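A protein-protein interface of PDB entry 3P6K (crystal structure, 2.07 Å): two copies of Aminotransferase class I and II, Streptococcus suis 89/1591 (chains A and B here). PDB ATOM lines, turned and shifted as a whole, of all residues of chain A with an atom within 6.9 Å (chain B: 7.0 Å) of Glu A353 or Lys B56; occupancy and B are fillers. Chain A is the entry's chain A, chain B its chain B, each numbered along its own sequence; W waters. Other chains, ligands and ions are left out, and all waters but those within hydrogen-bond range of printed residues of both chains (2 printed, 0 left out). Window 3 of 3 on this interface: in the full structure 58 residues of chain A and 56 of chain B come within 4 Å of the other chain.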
ATOM      1  N   ASP A  23      -7.788   6.480 -30.320  1.00  0.00           N
ATOM      2  CA  ASP A  23      -8.329   6.455 -31.693  1.00  0.00           C
ATOM      3  C   ASP A  23      -8.578   7.866 -32.219  1.00  0.00           C
ATOM      4  O   ASP A  23      -9.594   8.503 -31.879  1.00  0.00           O
ATOM      5  CB  ASP A  23      -9.622   5.610 -31.775  1.00  0.00           C
ATOM      6  CG  ASP A  23     -10.273   5.619 -33.186  1.00  0.00           C
ATOM      7  OD1 ASP A  23      -9.558   5.661 -34.221  1.00  0.00           O
ATOM      8  OD2 ASP A  23     -11.527   5.571 -33.255  1.00  0.00           O
ATOM      9  N   ILE A  24      -7.643   8.338 -33.053  1.00  0.00           N
ATOM     10  CA  ILE A  24      -7.774   9.624 -33.762  1.00  0.00           C
ATOM     11  C   ILE A  24      -7.814   9.346 -35.281  1.00  0.00           C
ATOM     12  O   ILE A  24      -7.278  10.112 -36.070  1.00  0.00           O
ATOM     13  CB  ILE A  24      -6.701  10.666 -33.319  1.00  0.00           C
ATOM     14  CG1 ILE A  24      -5.270  10.129 -33.445  1.00  0.00           C
ATOM     15  CG2 ILE A  24      -6.943  11.071 -31.873  1.00  0.00           C
ATOM     16  CD1 ILE A  24      -4.183  11.170 -33.145  1.00  0.00           C
ATOM     17  N   SER A  30     -17.604  13.046 -31.547  1.00  0.00           N
ATOM     18  CA  SER A  30     -17.958  12.296 -30.311  1.00  0.00           C
ATOM     19  C   SER A  30     -19.453  12.041 -30.117  1.00  0.00           C
ATOM     20  O   SER A  30     -20.205  12.931 -29.730  1.00  0.00           O
ATOM     21  CB  SER A  30     -17.399  12.992 -29.071  1.00  0.00           C
ATOM     22  OG  SER A  30     -17.923  14.303 -28.962  1.00  0.00           O
ATOM     23  N   SER A  31     -19.848  10.807 -30.393  1.00  0.00           N
ATOM     24  CA  SER A  31     -21.236  10.406 -30.409  1.00  0.00           C
ATOM     25  C   SER A  31     -22.016  10.634 -29.121  1.00  0.00           C
ATOM     26  O   SER A  31     -21.464  10.618 -28.040  1.00  0.00           O
ATOM     27  CB  SER A  31     -21.338   8.920 -30.777  1.00  0.00           C
ATOM     28  OG  SER A  31     -20.724   8.700 -32.034  1.00  0.00           O
ATOM     29  N   LEU A  32     -23.317  10.824 -29.300  1.00  0.00           N
ATOM     30  CA  LEU A  32     -24.244  11.011 -28.214  1.00  0.00           C
ATOM     31  C   LEU A  32     -24.791   9.667 -27.749  1.00  0.00           C
ATOM     32  O   LEU A  32     -24.870   8.713 -28.540  1.00  0.00           O
ATOM     33  CB  LEU A  32     -25.433  11.861 -28.697  1.00  0.00           C
ATOM     34  CG  LEU A  32     -25.212  13.320 -29.069  1.00  0.00           C
ATOM     35  CD1 LEU A  32     -26.495  13.867 -29.666  1.00  0.00           C
ATOM     36  CD2 LEU A  32     -24.800  14.134 -27.810  1.00  0.00           C
ATOM     37  N   THR A  33     -25.142   9.586 -26.465  1.00  0.00           N
ATOM     38  CA  THR A  33     -25.955   8.475 -25.947  1.00  0.00           C
ATOM     39  C   THR A  33     -27.393   8.974 -26.092  1.00  0.00           C
ATOM     40  O   THR A  33     -27.602  10.175 -26.270  1.00  0.00           O
ATOM     41  CB  THR A  33     -25.735   8.144 -24.442  1.00  0.00           C
ATOM     42  OG1 THR A  33     -26.135   9.260 -23.638  1.00  0.00           O
ATOM     43  CG2 THR A  33     -24.294   7.743 -24.132  1.00  0.00           C
ATOM     44  N   LEU A  34     -28.382   8.088 -25.993  1.00  0.00           N
ATOM     45  CA  LEU A  34     -29.787   8.544 -26.035  1.00  0.00           C
ATOM     46  C   LEU A  34     -30.086   9.498 -24.842  1.00  0.00           C
ATOM     47  O   LEU A  34     -30.764  10.512 -25.029  1.00  0.00           O
ATOM     48  CB  LEU A  34     -30.794   7.371 -26.081  1.00  0.00           C
ATOM     49  CG  LEU A  34     -32.258   7.710 -26.408  1.00  0.00           C
ATOM     50  CD1 LEU A  34     -32.410   8.364 -27.798  1.00  0.00           C
ATOM     51  CD2 LEU A  34     -33.107   6.464 -26.334  1.00  0.00           C
ATOM     52  N   GLU A  36     -27.990  11.567 -23.304  1.00  0.00           N
ATOM     53  CA  GLU A  36     -27.380  12.840 -23.661  1.00  0.00           C
ATOM     54  C   GLU A  36     -28.283  13.630 -24.589  1.00  0.00           C
ATOM     55  O   GLU A  36     -28.408  14.842 -24.414  1.00  0.00           O
ATOM     56  CB  GLU A  36     -26.056  12.709 -24.399  1.00  0.00           C
ATOM     57  CG  GLU A  36     -24.795  12.457 -23.614  1.00  0.00           C
ATOM     58  CD  GLU A  36     -23.626  12.486 -24.578  1.00  0.00           C
ATOM     59  OE1 GLU A  36     -23.122  11.403 -24.962  1.00  0.00           O
ATOM     60  OE2 GLU A  36     -23.299  13.604 -25.041  1.00  0.00           O
ATOM     61  N   GLY A 228     -25.094   5.733 -34.880  1.00  0.00           N
ATOM     62  CA  GLY A 228     -25.758   4.516 -34.434  1.00  0.00           C
ATOM     63  C   GLY A 228     -27.219   4.319 -34.770  1.00  0.00           C
ATOM     64  O   GLY A 228     -27.695   3.232 -34.574  1.00  0.00           O
ATOM     65  N   ILE A 280     -16.910  21.732 -29.687  1.00  0.00           N
ATOM     66  CA  ILE A 280     -15.973  20.588 -29.688  1.00  0.00           C
ATOM     67  C   ILE A 280     -14.939  20.774 -30.801  1.00  0.00           C
ATOM     68  O   ILE A 280     -13.728  20.703 -30.542  1.00  0.00           O
ATOM     69  CB  ILE A 280     -16.658  19.217 -29.892  1.00  0.00           C
ATOM     70  CG1 ILE A 280     -17.530  18.855 -28.685  1.00  0.00           C
ATOM     71  CG2 ILE A 280     -15.611  18.117 -30.097  1.00  0.00           C
ATOM     72  CD1 ILE A 280     -18.365  17.546 -28.894  1.00  0.00           C
ATOM     73  N   ASN A 284     -11.022  21.625 -30.150  1.00  0.00           N
ATOM     74  CA  ASN A 284     -10.090  20.570 -30.589  1.00  0.00           C
ATOM     75  C   ASN A 284      -9.186  20.998 -31.753  1.00  0.00           C
ATOM     76  O   ASN A 284      -8.017  20.584 -31.815  1.00  0.00           O
ATOM     77  CB  ASN A 284     -10.817  19.246 -30.904  1.00  0.00           C
ATOM     78  CG  ASN A 284     -11.281  18.492 -29.652  1.00  0.00           C
ATOM     79  OD1 ASN A 284     -11.184  18.976 -28.521  1.00  0.00           O
ATOM     80  ND2 ASN A 284     -11.772  17.285 -29.864  1.00  0.00           N
ATOM     81  N   PHE A 350     -10.014  14.616 -35.342  1.00  0.00           N
ATOM     82  CA  PHE A 350      -9.740  15.316 -34.078  1.00  0.00           C
ATOM     83  C   PHE A 350     -10.984  15.680 -33.272  1.00  0.00           C
ATOM     84  O   PHE A 350     -10.843  16.266 -32.213  1.00  0.00           O
ATOM     85  CB  PHE A 350      -8.884  16.573 -34.339  1.00  0.00           C
ATOM     86  CG  PHE A 350      -9.570  17.596 -35.172  1.00  0.00           C
ATOM     87  CD1 PHE A 350      -9.437  17.583 -36.569  1.00  0.00           C
ATOM     88  CD2 PHE A 350     -10.388  18.557 -34.579  1.00  0.00           C
ATOM     89  CE1 PHE A 350     -10.097  18.520 -37.345  1.00  0.00           C
ATOM     90  CE2 PHE A 350     -11.062  19.494 -35.355  1.00  0.00           C
ATOM     91  CZ  PHE A 350     -10.914  19.480 -36.731  1.00  0.00           C
ATOM     92  N   ALA A 351     -12.179  15.328 -33.742  1.00  0.00           N
ATOM     93  CA  ALA A 351     -13.423  15.601 -33.009  1.00  0.00           C
ATOM     94  C   ALA A 351     -13.816  14.496 -31.977  1.00  0.00           C
ATOM     95  O   ALA A 351     -15.000  14.355 -31.652  1.00  0.00           O
ATOM     96  CB  ALA A 351     -14.555  15.849 -33.990  1.00  0.00           C
ATOM     97  N   CYS A 352     -12.834  13.730 -31.476  1.00  0.00           N
ATOM     98  CA  CYS A 352     -13.019  12.718 -30.409  1.00  0.00           C
ATOM     99  C   CYS A 352     -12.989  13.441 -29.046  1.00  0.00           C
ATOM    100  O   CYS A 352     -12.824  14.658 -29.023  1.00  0.00           O
ATOM    101  CB  CYS A 352     -11.910  11.647 -30.491  1.00  0.00           C
ATOM    102  SG  CYS A 352     -10.163  12.324 -30.484  1.00  0.00           S
ATOM    103  N   GLU A 353     -13.152  12.728 -27.921  1.00  0.00           N
ATOM    104  CA  GLU A 353     -13.097  13.363 -26.561  1.00  0.00           C
ATOM    105  C   GLU A 353     -11.738  14.096 -26.413  1.00  0.00           C
ATOM    106  O   GLU A 353     -10.684  13.511 -26.713  1.00  0.00           O
ATOM    107  CB  GLU A 353     -13.330  12.327 -25.420  1.00  0.00           C
ATOM    108  CG  GLU A 353     -14.753  11.642 -25.426  1.00  0.00           C
ATOM    109  CD  GLU A 353     -14.883  10.346 -24.543  1.00  0.00           C
ATOM    110  OE1 GLU A 353     -14.062  10.128 -23.618  1.00  0.00           O
ATOM    111  OE2 GLU A 353     -15.832   9.535 -24.787  1.00  0.00           O
ATOM    112  N   GLN A 354     -11.779  15.376 -26.004  1.00  0.00           N
ATOM    113  CA  GLN A 354     -10.589  16.264 -25.933  1.00  0.00           C
ATOM    114  C   GLN A 354      -9.310  15.635 -25.377  1.00  0.00           C
ATOM    115  O   GLN A 354      -8.232  15.837 -25.945  1.00  0.00           O
ATOM    116  CB  GLN A 354     -10.894  17.585 -25.187  1.00  0.00           C
ATOM    117  CG  GLN A 354      -9.697  18.584 -25.145  1.00  0.00           C
ATOM    118  CD  GLN A 354     -10.045  19.958 -24.590  1.00  0.00           C
ATOM    119  OE1 GLN A 354     -10.982  20.612 -25.038  1.00  0.00           O
ATOM    120  NE2 GLN A 354      -9.255  20.415 -23.641  1.00  0.00           N
ATOM    121  N   GLU A 355      -9.442  14.887 -24.281  1.00  0.00           N
ATOM    122  CA  GLU A 355      -8.295  14.217 -23.627  1.00  0.00           C
ATOM    123  C   GLU A 355      -7.628  13.172 -24.541  1.00  0.00           C
ATOM    124  O   GLU A 355      -6.394  13.031 -24.517  1.00  0.00           O
ATOM    125  CB  GLU A 355      -8.759  13.529 -22.349  1.00  0.00           C
ATOM    126  CG  GLU A 355      -7.643  12.901 -21.481  1.00  0.00           C
ATOM    127  CD  GLU A 355      -8.051  11.594 -20.805  1.00  0.00           C
ATOM    128  OE1 GLU A 355      -9.177  11.078 -21.053  1.00  0.00           O
ATOM    129  OE2 GLU A 355      -7.212  11.065 -20.039  1.00  0.00           O
ATOM    130  N   THR A 356      -8.449  12.438 -25.305  1.00  0.00           N
ATOM    131  CA  THR A 356      -7.978  11.404 -26.252  1.00  0.00           C
ATOM    132  C   THR A 356      -7.080  12.017 -27.339  1.00  0.00           C
ATOM    133  O   THR A 356      -6.010  11.470 -27.645  1.00  0.00           O
ATOM    134  CB  THR A 356      -9.161  10.649 -26.904  1.00  0.00           C
ATOM    135  OG1 THR A 356     -10.024  10.172 -25.865  1.00  0.00           O
ATOM    136  CG2 THR A 356      -8.681   9.478 -27.774  1.00  0.00           C
ATOM    137  N   LEU A 357      -7.528  13.141 -27.902  1.00  0.00           N
ATOM    138  CA  LEU A 357      -6.748  13.915 -28.871  1.00  0.00           C
ATOM    139  C   LEU A 357      -5.417  14.383 -28.248  1.00  0.00           C
ATOM    140  O   LEU A 357      -4.368  14.172 -28.855  1.00  0.00           O
ATOM    141  CB  LEU A 357      -7.549  15.122 -29.369  1.00  0.00           C
ATOM    142  CG  LEU A 357      -6.886  16.114 -30.325  1.00  0.00           C
ATOM    143  CD1 LEU A 357      -6.453  15.412 -31.600  1.00  0.00           C
ATOM    144  CD2 LEU A 357      -7.849  17.239 -30.614  1.00  0.00           C
ATOM    145  N   ILE A 358      -5.471  14.970 -27.043  1.00  0.00           N
ATOM    146  CA  ILE A 358      -4.265  15.469 -26.319  1.00  0.00           C
ATOM    147  C   ILE A 358      -3.230  14.374 -26.080  1.00  0.00           C
ATOM    148  O   ILE A 358      -2.066  14.536 -26.432  1.00  0.00           O
ATOM    149  CB  ILE A 358      -4.616  16.150 -24.950  1.00  0.00           C
ATOM    150  CG1 ILE A 358      -5.363  17.474 -25.188  1.00  0.00           C
ATOM    151  CG2 ILE A 358      -3.340  16.465 -24.138  1.00  0.00           C
ATOM    152  CD1 ILE A 358      -5.983  18.096 -23.937  1.00  0.00           C
ATOM    153  N   LYS B  51     -30.163   0.200 -19.930  1.00  0.00           N
ATOM    154  CA  LYS B  51     -29.085  -0.309 -20.798  1.00  0.00           C
ATOM    155  C   LYS B  51     -28.975   0.600 -22.057  1.00  0.00           C
ATOM    156  O   LYS B  51     -27.893   1.136 -22.352  1.00  0.00           O
ATOM    157  CB  LYS B  51     -29.310  -1.792 -21.215  1.00  0.00           C
ATOM    158  CG  LYS B  51     -28.149  -2.448 -22.034  1.00  0.00           C
ATOM    159  CD  LYS B  51     -28.382  -3.933 -22.483  1.00  0.00           C
ATOM    160  CE  LYS B  51     -27.059  -4.531 -23.022  1.00  0.00           C
ATOM    161  NZ  LYS B  51     -27.059  -5.733 -23.981  1.00  0.00           N
ATOM    162  N   LEU B  52     -30.105   0.813 -22.732  1.00  0.00           N
ATOM    163  CA  LEU B  52     -30.167   1.569 -23.998  1.00  0.00           C
ATOM    164  C   LEU B  52     -29.632   2.985 -23.881  1.00  0.00           C
ATOM    165  O   LEU B  52     -28.719   3.373 -24.611  1.00  0.00           O
ATOM    166  CB  LEU B  52     -31.616   1.646 -24.522  1.00  0.00           C
ATOM    167  CG  LEU B  52     -31.923   2.493 -25.774  1.00  0.00           C
ATOM    168  CD1 LEU B  52     -31.068   2.060 -26.990  1.00  0.00           C
ATOM    169  CD2 LEU B  52     -33.392   2.429 -26.070  1.00  0.00           C
ATOM    170  N   GLN B  53     -30.176   3.716 -22.917  1.00  0.00           N
ATOM    171  CA  GLN B  53     -29.900   5.138 -22.784  1.00  0.00           C
ATOM    172  C   GLN B  53     -28.473   5.553 -22.405  1.00  0.00           C
ATOM    173  O   GLN B  53     -28.120   6.697 -22.627  1.00  0.00           O
ATOM    174  CB  GLN B  53     -30.929   5.809 -21.898  1.00  0.00           C
ATOM    175  CG  GLN B  53     -30.796   5.617 -20.417  1.00  0.00           C
ATOM    176  CD  GLN B  53     -31.933   6.281 -19.681  1.00  0.00           C
ATOM    177  OE1 GLN B  53     -32.928   6.685 -20.280  1.00  0.00           O
ATOM    178  NE2 GLN B  53     -31.781   6.421 -18.380  1.00  0.00           N
ATOM    179  N   GLY B  54     -27.706   4.652 -21.800  1.00  0.00           N
ATOM    180  CA  GLY B  54     -26.292   4.880 -21.543  1.00  0.00           C
ATOM    181  C   GLY B  54     -25.401   4.339 -22.667  1.00  0.00           C
ATOM    182  O   GLY B  54     -24.187   4.447 -22.582  1.00  0.00           O
ATOM    183  N   THR B  55     -25.982   3.762 -23.723  1.00  0.00           N
ATOM    184  CA  THR B  55     -25.194   3.199 -24.828  1.00  0.00           C
ATOM    185  C   THR B  55     -24.901   4.298 -25.847  1.00  0.00           C
ATOM    186  O   THR B  55     -25.813   4.979 -26.293  1.00  0.00           O
ATOM    187  CB  THR B  55     -25.900   1.988 -25.498  1.00  0.00           C
ATOM    188  OG1 THR B  55     -26.183   1.003 -24.499  1.00  0.00           O
ATOM    189  CG2 THR B  55     -25.007   1.363 -26.542  1.00  0.00           C
ATOM    190  N   LYS B  56     -23.627   4.511 -26.168  1.00  0.00           N
ATOM    191  CA  LYS B  56     -23.256   5.486 -27.209  1.00  0.00           C
ATOM    192  C   LYS B  56     -23.877   5.072 -28.529  1.00  0.00           C
ATOM    193  O   LYS B  56     -23.818   3.891 -28.920  1.00  0.00           O
ATOM    194  CB  LYS B  56     -21.731   5.618 -27.394  1.00  0.00           C
ATOM    195  CG  LYS B  56     -21.022   6.340 -26.297  1.00  0.00           C
ATOM    196  CD  LYS B  56     -19.573   6.641 -26.689  1.00  0.00           C
ATOM    197  CE  LYS B  56     -18.841   7.393 -25.628  1.00  0.00           C
ATOM    198  NZ  LYS B  56     -17.451   7.715 -26.040  1.00  0.00           N
ATOM    199  N   LEU B  57     -24.489   6.042 -29.210  1.00  0.00           N
ATOM    200  CA  LEU B  57     -25.040   5.842 -30.546  1.00  0.00           C
ATOM    201  C   LEU B  57     -23.943   6.160 -31.559  1.00  0.00           C
ATOM    202  O   LEU B  57     -24.129   6.954 -32.479  1.00  0.00           O
ATOM    203  CB  LEU B  57     -26.324   6.670 -30.750  1.00  0.00           C
ATOM    204  CG  LEU B  57     -27.479   6.329 -29.787  1.00  0.00           C
ATOM    205  CD1 LEU B  57     -28.657   7.278 -29.978  1.00  0.00           C
ATOM    206  CD2 LEU B  57     -27.958   4.887 -29.936  1.00  0.00           C
ATOM    207  N   ASN B  58     -22.789   5.507 -31.393  1.00  0.00           N
ATOM    208  CA  ASN B  58     -21.668   5.604 -32.309  1.00  0.00           C
ATOM    209  C   ASN B  58     -21.897   4.507 -33.320  1.00  0.00           C
ATOM    210  O   ASN B  58     -23.003   3.940 -33.392  1.00  0.00           O
ATOM    211  CB  ASN B  58     -20.300   5.559 -31.566  1.00  0.00           C
ATOM    212  CG  ASN B  58     -20.073   4.294 -30.720  1.00  0.00           C
ATOM    213  OD1 ASN B  58     -20.783   3.301 -30.823  1.00  0.00           O
ATOM    214  ND2 ASN B  58     -19.077   4.368 -29.845  1.00  0.00           N
ATOM    215  N   TYR B  59     -20.894   4.178 -34.132  1.00  0.00           N
ATOM    216  CA  TYR B  59     -21.048   3.050 -35.071  1.00  0.00           C
ATOM    217  C   TYR B  59     -21.266   1.673 -34.408  1.00  0.00           C
ATOM    218  O   TYR B  59     -21.787   0.755 -35.058  1.00  0.00           O
ATOM    219  CB  TYR B  59     -19.928   3.019 -36.116  1.00  0.00           C
ATOM    220  CG  TYR B  59     -20.056   4.142 -37.103  1.00  0.00           C
ATOM    221  CD1 TYR B  59     -20.935   4.035 -38.180  1.00  0.00           C
ATOM    222  CD2 TYR B  59     -19.328   5.316 -36.968  1.00  0.00           C
ATOM    223  CE1 TYR B  59     -21.083   5.081 -39.105  1.00  0.00           C
ATOM    224  CE2 TYR B  59     -19.465   6.360 -37.906  1.00  0.00           C
ATOM    225  CZ  TYR B  59     -20.369   6.218 -38.966  1.00  0.00           C
ATOM    226  OH  TYR B  59     -20.528   7.224 -39.905  1.00  0.00           O
ATOM    227  N   GLY B  60     -20.882   1.532 -33.131  1.00  0.00           N
ATOM    228  CA  GLY B  60     -21.161   0.322 -32.374  1.00  0.00           C
ATOM    229  C   GLY B  60     -20.507  -0.924 -32.929  1.00  0.00           C
ATOM    230  O   GLY B  60     -19.367  -0.866 -33.409  1.00  0.00           O
ATOM    231  N   VAL B 257     -27.452   0.570 -33.501  1.00  0.00           N
ATOM    232  CA  VAL B 257     -27.127   0.196 -32.114  1.00  0.00           C
ATOM    233  C   VAL B 257     -28.381  -0.286 -31.372  1.00  0.00           C
ATOM    234  O   VAL B 257     -28.351  -1.344 -30.760  1.00  0.00           O
ATOM    235  CB  VAL B 257     -26.424   1.337 -31.339  1.00  0.00           C
ATOM    236  CG1 VAL B 257     -26.254   1.011 -29.887  1.00  0.00           C
ATOM    237  CG2 VAL B 257     -25.065   1.665 -32.005  1.00  0.00           C
HETATM  238  O   HOH W   1     -30.248   1.894 -33.863  1.00  0.00           O
HETATM  239  O   HOH W   2     -28.359   5.306 -26.461  1.00  0.00           O
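CB of Ser A31 touches O of Leu B57, 3.8 Å away. Ser A31 touches Asn B58. Leu A32 touches Lys B56. Thr A33 touches Gly B54 (CG2 to O, 3.6 Å). Thr B55 touches Thr A33 (O to CA, 3.5 Å). Thr A33 touches Lys B56. Gln B53 touches Leu A34 (O to N, 3.7 Å).
OG1 of Thr A33 lies within hydrogen-bond range of N of Glu A36, 3.0 Å away. The backbone carbonyl oxygen (O) of Lys B51 sits at hydrogen-bond distance from the side-chain hydroxyl (OG1) of Thr B55 (2.7 Å). The backbone carbonyl oxygen (O) of Leu B52 lies close to the side-chain hydroxyl (OG1) of Thr B55, 3.5 Å away. The side-chain amide oxygen (OD1) of Asn B58 lies within hydrogen-bond range of the backbone NH (N) of Gly B60, 2.9 Å away.
Of the printed residues of chain B, Ser A31 touches Leu B57 and Asn B58. Of the printed residues of chain B, Leu A34 touches Gln B53. Printed residues of chain A within 4 Å of Gln B53: Thr A33 and Leu A34. Lys B56 touches just these residues of chain A: Leu A32 (3.8 Å), Thr A33 (3.9 Å) and Glu A353 (2.7 Å). Printed residues of chain A within 4 Å of Leu B57: Ser A31 (3.8 Å), Leu A32 (2.8 Å) and Gly A228 (2.9 Å). Tyr B59 touches none of the printed residues of chain A. The nearest printed residue of chain B that does not touch Ser A31 is Lys B56 (4.6 Å).
Of the 20 printed residues of chain A, 6 touch a printed residue of chain B. Hydrophobic or aromatic side chains of chain B that line the printed part of chain A: Leu B57 and Val B257. Among the printed residues, 13 pairs touch across the chains.
Water W2 lies within hydrogen-bond range of O of Thr B55 (2.6 Å), O of Leu B52 (2.7 Å) and N of Leu A34 (2.8 Å). Water W1 bridges the backbone carbonyl oxygen of Gly A228 (3.0 Å) and the backbone NH of Val B257 (3.1 Å).
No position is printed for both chains. Of the 13 pairs that touch across the chains among the printed residues, none has its exchanged pair printed and touching as well.
N of Val B257 is in hydrogen-bond range of O of Gly A228, 2.9 Å away. The backbone carbonyl oxygen (O) of Leu A32 is in hydrogen-bond range of the backbone NH (N) of Leu B57 (2.8 Å). The side-chain amino group of Lys B56 is in salt-bridge range of the side-chain carboxylate of Glu A353, at 2.7 Å. O of Gln B53 lies close to OG1 of Thr A33 (3.4 Å). The backbone carbonyl oxygen of Leu B57 lies within hydrogen-bond range of the backbone NH of Gly A228 (2.9 Å). The backbone NH (N) of Gly A228 lies close to the backbone carbonyl oxygen (O) of Asn B58, 3.1 Å away.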
